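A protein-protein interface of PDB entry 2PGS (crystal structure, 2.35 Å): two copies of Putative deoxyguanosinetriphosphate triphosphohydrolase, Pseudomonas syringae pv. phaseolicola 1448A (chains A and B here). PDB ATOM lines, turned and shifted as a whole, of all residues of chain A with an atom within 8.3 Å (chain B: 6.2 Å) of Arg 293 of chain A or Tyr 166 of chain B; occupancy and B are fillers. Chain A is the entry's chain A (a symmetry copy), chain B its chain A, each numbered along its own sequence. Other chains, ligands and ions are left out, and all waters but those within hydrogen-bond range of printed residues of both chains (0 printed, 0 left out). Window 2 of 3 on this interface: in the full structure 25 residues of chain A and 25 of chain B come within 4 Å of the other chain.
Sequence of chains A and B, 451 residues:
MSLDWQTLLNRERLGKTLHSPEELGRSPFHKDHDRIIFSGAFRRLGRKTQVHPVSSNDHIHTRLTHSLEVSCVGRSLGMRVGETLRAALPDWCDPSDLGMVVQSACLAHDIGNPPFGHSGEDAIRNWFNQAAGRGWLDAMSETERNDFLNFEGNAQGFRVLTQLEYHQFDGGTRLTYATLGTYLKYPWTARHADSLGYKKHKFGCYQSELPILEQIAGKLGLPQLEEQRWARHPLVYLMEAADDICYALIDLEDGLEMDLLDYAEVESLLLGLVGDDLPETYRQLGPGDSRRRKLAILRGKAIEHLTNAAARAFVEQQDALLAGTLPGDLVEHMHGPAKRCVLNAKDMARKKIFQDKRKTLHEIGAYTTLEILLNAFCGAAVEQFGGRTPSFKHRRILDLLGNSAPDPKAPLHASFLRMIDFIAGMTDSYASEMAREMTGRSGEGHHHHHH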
ATOM      1  N   GLU A 253     -14.292 -16.480  20.227  1.00  0.00           N
ATOM      2  CA  GLU A 253     -14.651 -15.754  21.425  1.00  0.00           C
ATOM      3  C   GLU A 253     -13.611 -15.886  22.541  1.00  0.00           C
ATOM      4  O   GLU A 253     -13.147 -14.880  23.066  1.00  0.00           O
ATOM      5  CB  GLU A 253     -16.017 -16.223  21.911  1.00  0.00           C
ATOM      6  CG  GLU A 253     -16.603 -15.372  23.006  1.00  0.00           C
ATOM      7  CD  GLU A 253     -18.045 -15.738  23.295  1.00  0.00           C
ATOM      8  OE1 GLU A 253     -18.292 -16.851  23.816  1.00  0.00           O
ATOM      9  OE2 GLU A 253     -18.929 -14.908  22.985  1.00  0.00           O
ATOM     10  N   ARG A 292     -17.569  -6.108  23.887  1.00  0.00           N
ATOM     11  CA  ARG A 292     -17.524  -7.563  24.018  1.00  0.00           C
ATOM     12  C   ARG A 292     -18.928  -8.144  24.016  1.00  0.00           C
ATOM     13  O   ARG A 292     -19.120  -9.334  23.753  1.00  0.00           O
ATOM     14  CB  ARG A 292     -16.841  -7.973  25.319  1.00  0.00           C
ATOM     15  N   ARG A 293     -19.902  -7.302  24.338  1.00  0.00           N
ATOM     16  CA  ARG A 293     -21.295  -7.726  24.371  1.00  0.00           C
ATOM     17  C   ARG A 293     -21.933  -7.418  23.035  1.00  0.00           C
ATOM     18  O   ARG A 293     -22.986  -7.951  22.692  1.00  0.00           O
ATOM     19  CB  ARG A 293     -22.025  -7.018  25.508  1.00  0.00           C
ATOM     20  N   LYS A 294     -21.271  -6.554  22.281  1.00  0.00           N
ATOM     21  CA  LYS A 294     -21.744  -6.196  20.961  1.00  0.00           C
ATOM     22  C   LYS A 294     -21.432  -7.415  20.099  1.00  0.00           C
ATOM     23  O   LYS A 294     -22.058  -7.647  19.065  1.00  0.00           O
ATOM     24  N   LEU A 295     -20.460  -8.198  20.558  1.00  0.00           N
ATOM     25  CA  LEU A 295     -20.037  -9.396  19.850  1.00  0.00           C
ATOM     26  C   LEU A 295     -20.923 -10.582  20.183  1.00  0.00           C
ATOM     27  O   LEU A 295     -21.247 -11.383  19.310  1.00  0.00           O
ATOM     28  CB  LEU A 295     -18.592  -9.748  20.204  1.00  0.00           C
ATOM     29  CG  LEU A 295     -18.081 -10.978  19.451  1.00  0.00           C
ATOM     30  CD1 LEU A 295     -17.961 -10.655  17.968  1.00  0.00           C
ATOM     31  CD2 LEU A 295     -16.748 -11.410  20.020  1.00  0.00           C
ATOM     32  N   ALA A 296     -21.298 -10.698  21.453  1.00  0.00           N
ATOM     33  CA  ALA A 296     -22.151 -11.790  21.891  1.00  0.00           C
ATOM     34  C   ALA A 296     -23.463 -11.681  21.126  1.00  0.00           C
ATOM     35  O   ALA A 296     -24.119 -12.687  20.842  1.00  0.00           O
ATOM     36  CB  ALA A 296     -22.393 -11.698  23.394  1.00  0.00           C
ATOM     37  N   ILE A 297     -23.836 -10.453  20.780  1.00  0.00           N
ATOM     38  CA  ILE A 297     -25.063 -10.220  20.033  1.00  0.00           C
ATOM     39  C   ILE A 297     -24.842 -10.644  18.584  1.00  0.00           C
ATOM     40  O   ILE A 297     -25.726 -11.232  17.959  1.00  0.00           O
ATOM     41  CB  ILE A 297     -25.486  -8.732  20.124  1.00  0.00           C
ATOM     42  CG1 ILE A 297     -25.846  -8.408  21.580  1.00  0.00           C
ATOM     43  CG2 ILE A 297     -26.673  -8.450  19.205  1.00  0.00           C
ATOM     44  CD1 ILE A 297     -26.239  -6.962  21.833  1.00  0.00           C
ATOM     45  N   LEU A 298     -23.662 -10.343  18.050  1.00  0.00           N
ATOM     46  CA  LEU A 298     -23.335 -10.764  16.691  1.00  0.00           C
ATOM     47  C   LEU A 298     -23.285 -12.294  16.702  1.00  0.00           C
ATOM     48  O   LEU A 298     -23.891 -12.951  15.856  1.00  0.00           O
ATOM     49  CB  LEU A 298     -21.965 -10.226  16.267  1.00  0.00           C
ATOM     50  CG  LEU A 298     -21.861  -8.786  15.769  1.00  0.00           C
ATOM     51  CD1 LEU A 298     -20.396  -8.418  15.548  1.00  0.00           C
ATOM     52  CD2 LEU A 298     -22.647  -8.647  14.470  1.00  0.00           C
ATOM     53  N   ARG A 299     -22.551 -12.840  17.672  1.00  0.00           N
ATOM     54  CA  ARG A 299     -22.395 -14.281  17.842  1.00  0.00           C
ATOM     55  C   ARG A 299     -23.778 -14.902  17.767  1.00  0.00           C
ATOM     56  O   ARG A 299     -23.992 -15.884  17.060  1.00  0.00           O
ATOM     57  CB  ARG A 299     -21.756 -14.582  19.206  1.00  0.00           C
ATOM     58  CG  ARG A 299     -21.357 -16.052  19.442  1.00  0.00           C
ATOM     59  CD  ARG A 299     -21.128 -16.326  20.933  1.00  0.00           C
ATOM     60  NE  ARG A 299     -22.362 -16.142  21.691  1.00  0.00           N
ATOM     61  CZ  ARG A 299     -22.417 -15.710  22.946  1.00  0.00           C
ATOM     62  NH1 ARG A 299     -21.304 -15.418  23.593  1.00  0.00           N
ATOM     63  NH2 ARG A 299     -23.588 -15.547  23.551  1.00  0.00           N
ATOM     64  N   GLY A 300     -24.721 -14.301  18.490  1.00  0.00           N
ATOM     65  CA  GLY A 300     -26.089 -14.788  18.497  1.00  0.00           C
ATOM     66  C   GLY A 300     -26.692 -14.846  17.108  1.00  0.00           C
ATOM     67  O   GLY A 300     -27.345 -15.826  16.748  1.00  0.00           O
ATOM     68  N   ILE A 303     -24.873 -17.510  14.872  1.00  0.00           N
ATOM     69  CA  ILE A 303     -25.348 -18.849  15.203  1.00  0.00           C
ATOM     70  C   ILE A 303     -26.674 -19.139  14.499  1.00  0.00           C
ATOM     71  O   ILE A 303     -26.852 -20.221  13.937  1.00  0.00           O
ATOM     72  CB  ILE A 303     -25.533 -19.018  16.739  1.00  0.00           C
ATOM     73  CG1 ILE A 303     -24.186 -18.835  17.438  1.00  0.00           C
ATOM     74  CG2 ILE A 303     -26.065 -20.410  17.072  1.00  0.00           C
ATOM     75  CD1 ILE A 303     -24.276 -18.842  18.941  1.00  0.00           C
ATOM     76  N   ASP B  34     -31.101 -21.249  25.661  1.00  0.00           N
ATOM     77  CA  ASP B  34     -29.825 -21.001  24.988  1.00  0.00           C
ATOM     78  C   ASP B  34     -29.114 -19.720  25.449  1.00  0.00           C
ATOM     79  O   ASP B  34     -27.891 -19.697  25.624  1.00  0.00           O
ATOM     80  CB  ASP B  34     -30.027 -20.955  23.467  1.00  0.00           C
ATOM     81  CG  ASP B  34     -30.438 -22.311  22.877  1.00  0.00           C
ATOM     82  OD1 ASP B  34     -30.593 -23.300  23.630  1.00  0.00           O
ATOM     83  OD2 ASP B  34     -30.609 -22.394  21.644  1.00  0.00           O
ATOM     84  N   ARG B  35     -29.860 -18.643  25.650  1.00  0.00           N
ATOM     85  CA  ARG B  35     -29.223 -17.405  26.084  1.00  0.00           C
ATOM     86  C   ARG B  35     -28.567 -17.589  27.435  1.00  0.00           C
ATOM     87  O   ARG B  35     -27.536 -16.980  27.726  1.00  0.00           O
ATOM     88  CB  ARG B  35     -30.242 -16.264  26.157  1.00  0.00           C
ATOM     89  CG  ARG B  35     -30.743 -15.837  24.790  1.00  0.00           C
ATOM     90  CD  ARG B  35     -31.703 -14.675  24.888  1.00  0.00           C
ATOM     91  NE  ARG B  35     -32.053 -14.176  23.561  1.00  0.00           N
ATOM     92  CZ  ARG B  35     -32.888 -13.168  23.340  1.00  0.00           C
ATOM     93  NH1 ARG B  35     -33.462 -12.546  24.358  1.00  0.00           N
ATOM     94  NH2 ARG B  35     -33.152 -12.789  22.102  1.00  0.00           N
ATOM     95  N   ILE B  36     -29.175 -18.417  28.273  1.00  0.00           N
ATOM     96  CA  ILE B  36     -28.618 -18.672  29.587  1.00  0.00           C
ATOM     97  C   ILE B  36     -27.369 -19.539  29.456  1.00  0.00           C
ATOM     98  O   ILE B  36     -26.353 -19.251  30.060  1.00  0.00           O
ATOM     99  CB  ILE B  36     -29.631 -19.381  30.481  1.00  0.00           C
ATOM    100  CG1 ILE B  36     -30.831 -18.463  30.703  1.00  0.00           C
ATOM    101  CG2 ILE B  36     -28.991 -19.743  31.814  1.00  0.00           C
ATOM    102  CD1 ILE B  36     -32.062 -19.181  31.241  1.00  0.00           C
ATOM    103  N   ILE B  37     -27.439 -20.577  28.635  1.00  0.00           N
ATOM    104  CA  ILE B  37     -26.303 -21.467  28.477  1.00  0.00           C
ATOM    105  C   ILE B  37     -25.071 -20.796  27.877  1.00  0.00           C
ATOM    106  O   ILE B  37     -23.947 -21.099  28.283  1.00  0.00           O
ATOM    107  CB  ILE B  37     -26.710 -22.743  27.681  1.00  0.00           C
ATOM    108  CG1 ILE B  37     -27.505 -23.658  28.627  1.00  0.00           C
ATOM    109  CG2 ILE B  37     -25.488 -23.463  27.129  1.00  0.00           C
ATOM    110  CD1 ILE B  37     -27.686 -25.040  28.139  1.00  0.00           C
ATOM    111  N   PHE B  38     -25.275 -19.874  26.939  1.00  0.00           N
ATOM    112  CA  PHE B  38     -24.149 -19.177  26.321  1.00  0.00           C
ATOM    113  C   PHE B  38     -23.601 -17.999  27.150  1.00  0.00           C
ATOM    114  O   PHE B  38     -22.511 -17.510  26.868  1.00  0.00           O
ATOM    115  CB  PHE B  38     -24.528 -18.676  24.911  1.00  0.00           C
ATOM    116  CG  PHE B  38     -24.477 -19.754  23.846  1.00  0.00           C
ATOM    117  CD1 PHE B  38     -25.478 -20.712  23.748  1.00  0.00           C
ATOM    118  CD2 PHE B  38     -23.405 -19.832  22.966  1.00  0.00           C
ATOM    119  CE1 PHE B  38     -25.407 -21.733  22.792  1.00  0.00           C
ATOM    120  CE2 PHE B  38     -23.328 -20.849  22.010  1.00  0.00           C
ATOM    121  CZ  PHE B  38     -24.336 -21.801  21.925  1.00  0.00           C
ATOM    122  N   SER B  39     -24.321 -17.560  28.179  1.00  0.00           N
ATOM    123  CA  SER B  39     -23.865 -16.414  28.960  1.00  0.00           C
ATOM    124  C   SER B  39     -22.613 -16.672  29.796  1.00  0.00           C
ATOM    125  O   SER B  39     -22.428 -17.754  30.370  1.00  0.00           O
ATOM    126  CB  SER B  39     -24.982 -15.915  29.877  1.00  0.00           C
ATOM    127  OG  SER B  39     -25.180 -16.825  30.953  1.00  0.00           O
ATOM    128  N   GLY B  40     -21.765 -15.652  29.879  1.00  0.00           N
ATOM    129  CA  GLY B  40     -20.535 -15.772  30.644  1.00  0.00           C
ATOM    130  C   GLY B  40     -20.808 -16.088  32.099  1.00  0.00           C
ATOM    131  O   GLY B  40     -20.032 -16.808  32.736  1.00  0.00           O
ATOM    132  N   LEU B 164     -27.183  -6.978  33.906  1.00  0.00           N
ATOM    133  CA  LEU B 164     -25.799  -7.206  33.513  1.00  0.00           C
ATOM    134  C   LEU B 164     -25.433  -7.947  32.217  1.00  0.00           C
ATOM    135  O   LEU B 164     -24.577  -7.477  31.486  1.00  0.00           O
ATOM    136  CB  LEU B 164     -25.057  -7.828  34.706  1.00  0.00           C
ATOM    137  CG  LEU B 164     -24.580  -6.881  35.822  1.00  0.00           C
ATOM    138  CD1 LEU B 164     -25.285  -5.543  35.739  1.00  0.00           C
ATOM    139  CD2 LEU B 164     -24.795  -7.516  37.175  1.00  0.00           C
ATOM    140  N   GLU B 165     -26.062  -9.076  31.915  1.00  0.00           N
ATOM    141  CA  GLU B 165     -25.718  -9.828  30.704  1.00  0.00           C
ATOM    142  C   GLU B 165     -26.270  -9.266  29.393  1.00  0.00           C
ATOM    143  O   GLU B 165     -27.302  -8.589  29.381  1.00  0.00           O
ATOM    144  CB  GLU B 165     -26.184 -11.284  30.844  1.00  0.00           C
ATOM    145  CG  GLU B 165     -25.470 -12.067  31.921  1.00  0.00           C
ATOM    146  CD  GLU B 165     -24.088 -12.551  31.497  1.00  0.00           C
ATOM    147  OE1 GLU B 165     -23.221 -12.696  32.379  1.00  0.00           O
ATOM    148  OE2 GLU B 165     -23.862 -12.809  30.297  1.00  0.00           O
ATOM    149  N   TYR B 166     -25.569  -9.564  28.298  1.00  0.00           N
ATOM    150  CA  TYR B 166     -25.953  -9.157  26.940  1.00  0.00           C
ATOM    151  C   TYR B 166     -26.264  -7.666  26.777  1.00  0.00           C
ATOM    152  O   TYR B 166     -25.352  -6.842  26.675  1.00  0.00           O
ATOM    153  CB  TYR B 166     -27.154  -9.998  26.467  1.00  0.00           C
ATOM    154  CG  TYR B 166     -26.864 -11.484  26.328  1.00  0.00           C
ATOM    155  CD1 TYR B 166     -26.075 -11.973  25.281  1.00  0.00           C
ATOM    156  CD2 TYR B 166     -27.363 -12.404  27.256  1.00  0.00           C
ATOM    157  CE1 TYR B 166     -25.785 -13.341  25.165  1.00  0.00           C
ATOM    158  CE2 TYR B 166     -27.085 -13.772  27.149  1.00  0.00           C
ATOM    159  CZ  TYR B 166     -26.295 -14.233  26.104  1.00  0.00           C
ATOM    160  OH  TYR B 166     -26.011 -15.579  26.005  1.00  0.00           O
ATOM    161  N   HIS B 167     -27.551  -7.329  26.738  1.00  0.00           N
ATOM    162  CA  HIS B 167     -27.988  -5.942  26.587  1.00  0.00           C
ATOM    163  C   HIS B 167     -27.928  -5.234  27.930  1.00  0.00           C
ATOM    164  O   HIS B 167     -28.950  -5.005  28.575  1.00  0.00           O
ATOM    165  CB  HIS B 167     -29.406  -5.919  26.032  1.00  0.00           C
ATOM    166  CG  HIS B 167     -29.512  -6.486  24.652  1.00  0.00           C
ATOM    167  ND1 HIS B 167     -29.203  -5.758  23.524  1.00  0.00           N
ATOM    168  CD2 HIS B 167     -29.859  -7.723  24.219  1.00  0.00           C
ATOM    169  CE1 HIS B 167     -29.358  -6.519  22.454  1.00  0.00           C
ATOM    170  NE2 HIS B 167     -29.755  -7.716  22.849  1.00  0.00           N
ATOM    171  N   GLN B 168     -26.716  -4.886  28.345  1.00  0.00           N
ATOM    172  CA  GLN B 168     -26.511  -4.243  29.630  1.00  0.00           C
ATOM    173  C   GLN B 168     -27.477  -3.095  29.896  1.00  0.00           C
ATOM    174  O   GLN B 168     -27.668  -2.213  29.061  1.00  0.00           O
ATOM    175  CB  GLN B 168     -25.069  -3.760  29.751  1.00  0.00           C
ATOM    176  CG  GLN B 168     -24.609  -3.606  31.189  1.00  0.00           C
ATOM    177  CD  GLN B 168     -23.148  -3.217  31.296  1.00  0.00           C
ATOM    178  OE1 GLN B 168     -22.416  -3.230  30.305  1.00  0.00           O
ATOM    179  NE2 GLN B 168     -22.710  -2.881  32.506  1.00  0.00           N
ATOM    180  N   GLY B 172     -31.075  -6.752  29.616  1.00  0.00           N
ATOM    181  CA  GLY B 172     -30.125  -7.803  29.917  1.00  0.00           C
ATOM    182  C   GLY B 172     -30.252  -8.993  28.995  1.00  0.00           C
ATOM    183  O   GLY B 172     -30.133  -8.870  27.770  1.00  0.00           O
ATOM    184  N   THR B 173     -30.489 -10.157  29.592  1.00  0.00           N
ATOM    185  CA  THR B 173     -30.632 -11.398  28.830  1.00  0.00           C
ATOM    186  C   THR B 173     -31.925 -11.379  28.005  1.00  0.00           C
ATOM    187  O   THR B 173     -32.124 -12.209  27.120  1.00  0.00           O
ATOM    188  CB  THR B 173     -30.622 -12.633  29.783  1.00  0.00           C
ATOM    189  OG1 THR B 173     -29.482 -12.561  30.647  1.00  0.00           O
ATOM    190  CG2 THR B 173     -30.493 -13.913  29.000  1.00  0.00           C
ATOM    191  N   ARG B 174     -32.795 -10.417  28.307  1.00  0.00           N
ATOM    192  CA  ARG B 174     -34.071 -10.260  27.614  1.00  0.00           C
ATOM    193  C   ARG B 174     -34.849 -11.561  27.494  1.00  0.00           C
ATOM    194  O   ARG B 174     -35.251 -11.976  26.409  1.00  0.00           O
ATOM    195  CB  ARG B 174     -33.858  -9.645  26.226  1.00  0.00           C
ATOM    196  CG  ARG B 174     -33.549  -8.163  26.284  1.00  0.00           C
ATOM    197  CD  ARG B 174     -33.355  -7.574  24.905  1.00  0.00           C
ATOM    198  NE  ARG B 174     -32.995  -6.164  24.988  1.00  0.00           N
ATOM    199  CZ  ARG B 174     -32.740  -5.390  23.939  1.00  0.00           C
ATOM    200  NH1 ARG B 174     -32.804  -5.887  22.709  1.00  0.00           N
ATOM    201  NH2 ARG B 174     -32.417  -4.115  24.124  1.00  0.00           N
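CB of Arg 293 of chain A touches O of Tyr 166 of chain B, 3.5 Å away. CD1 of Ile 297 of chain A touches CE1 of His 167 of chain B, at 3.2 Å. Phe 38 of chain B touches Arg 299 of chain A. CE2 of Phe 38 of chain B touches CD1 of Ile 303 of chain A, 3.8 Å away.
Of chain B, only Tyr 166 comes within 4 Å of Arg 293 of chain A. Printed residues of chain B within 4 Å of Ile 303 of chain A: Phe 38. Of the printed residues of chain B, Arg 299 of chain A touches Phe 38 and Tyr 166. Of the printed residues of chain A, Phe 38 of chain B touches Arg 299 and Ile 303. Printed residues of chain A within 4 Å of His 167 of chain B: Ile 297. Printed residues of chain B within 4 Å of Ile 297 of chain A: His 167 (3.2 Å). Gly 300 of chain A touches none of the printed residues of chain B.
No position is printed for both chains. Of the 5 pairs that touch across the chains among the printed residues, none has its exchanged pair printed and touching as well.
OH of Tyr 166 of chain B sits at hydrogen-bond distance from NH2 of Arg 299 of chain A (3.4 Å).
The side-chain carboxylate (OE2) of Glu 253 of chain A is in salt-bridge range of the guanidinium group (NH1) of Arg 299 of chain A (2.5 Å). The side-chain hydroxyl (OH) of Tyr 166 of chain B sits at hydrogen-bond distance from the backbone NH (N) of Ser 39 of chain B (3.4 Å). The backbone carbonyl oxygen of His 167 of chain B lies within hydrogen-bond range of the backbone NH of Gly 172 of chain B, at 2.9 Å. The side-chain hydroxyl of Tyr 166 of chain B is in hydrogen-bond range of the backbone carbonyl oxygen of Arg 35 of chain B (2.7 Å).
Of the 11 printed residues of chain A, 4 touch a printed residue of chain B. Hydrophobic or aromatic side chains of chain A within 4 Å of the printed part of chain B: Ile 297 and Ile 303. Along chain B the printed residues that touch a printed residue of chain A span positions 38 to 167.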
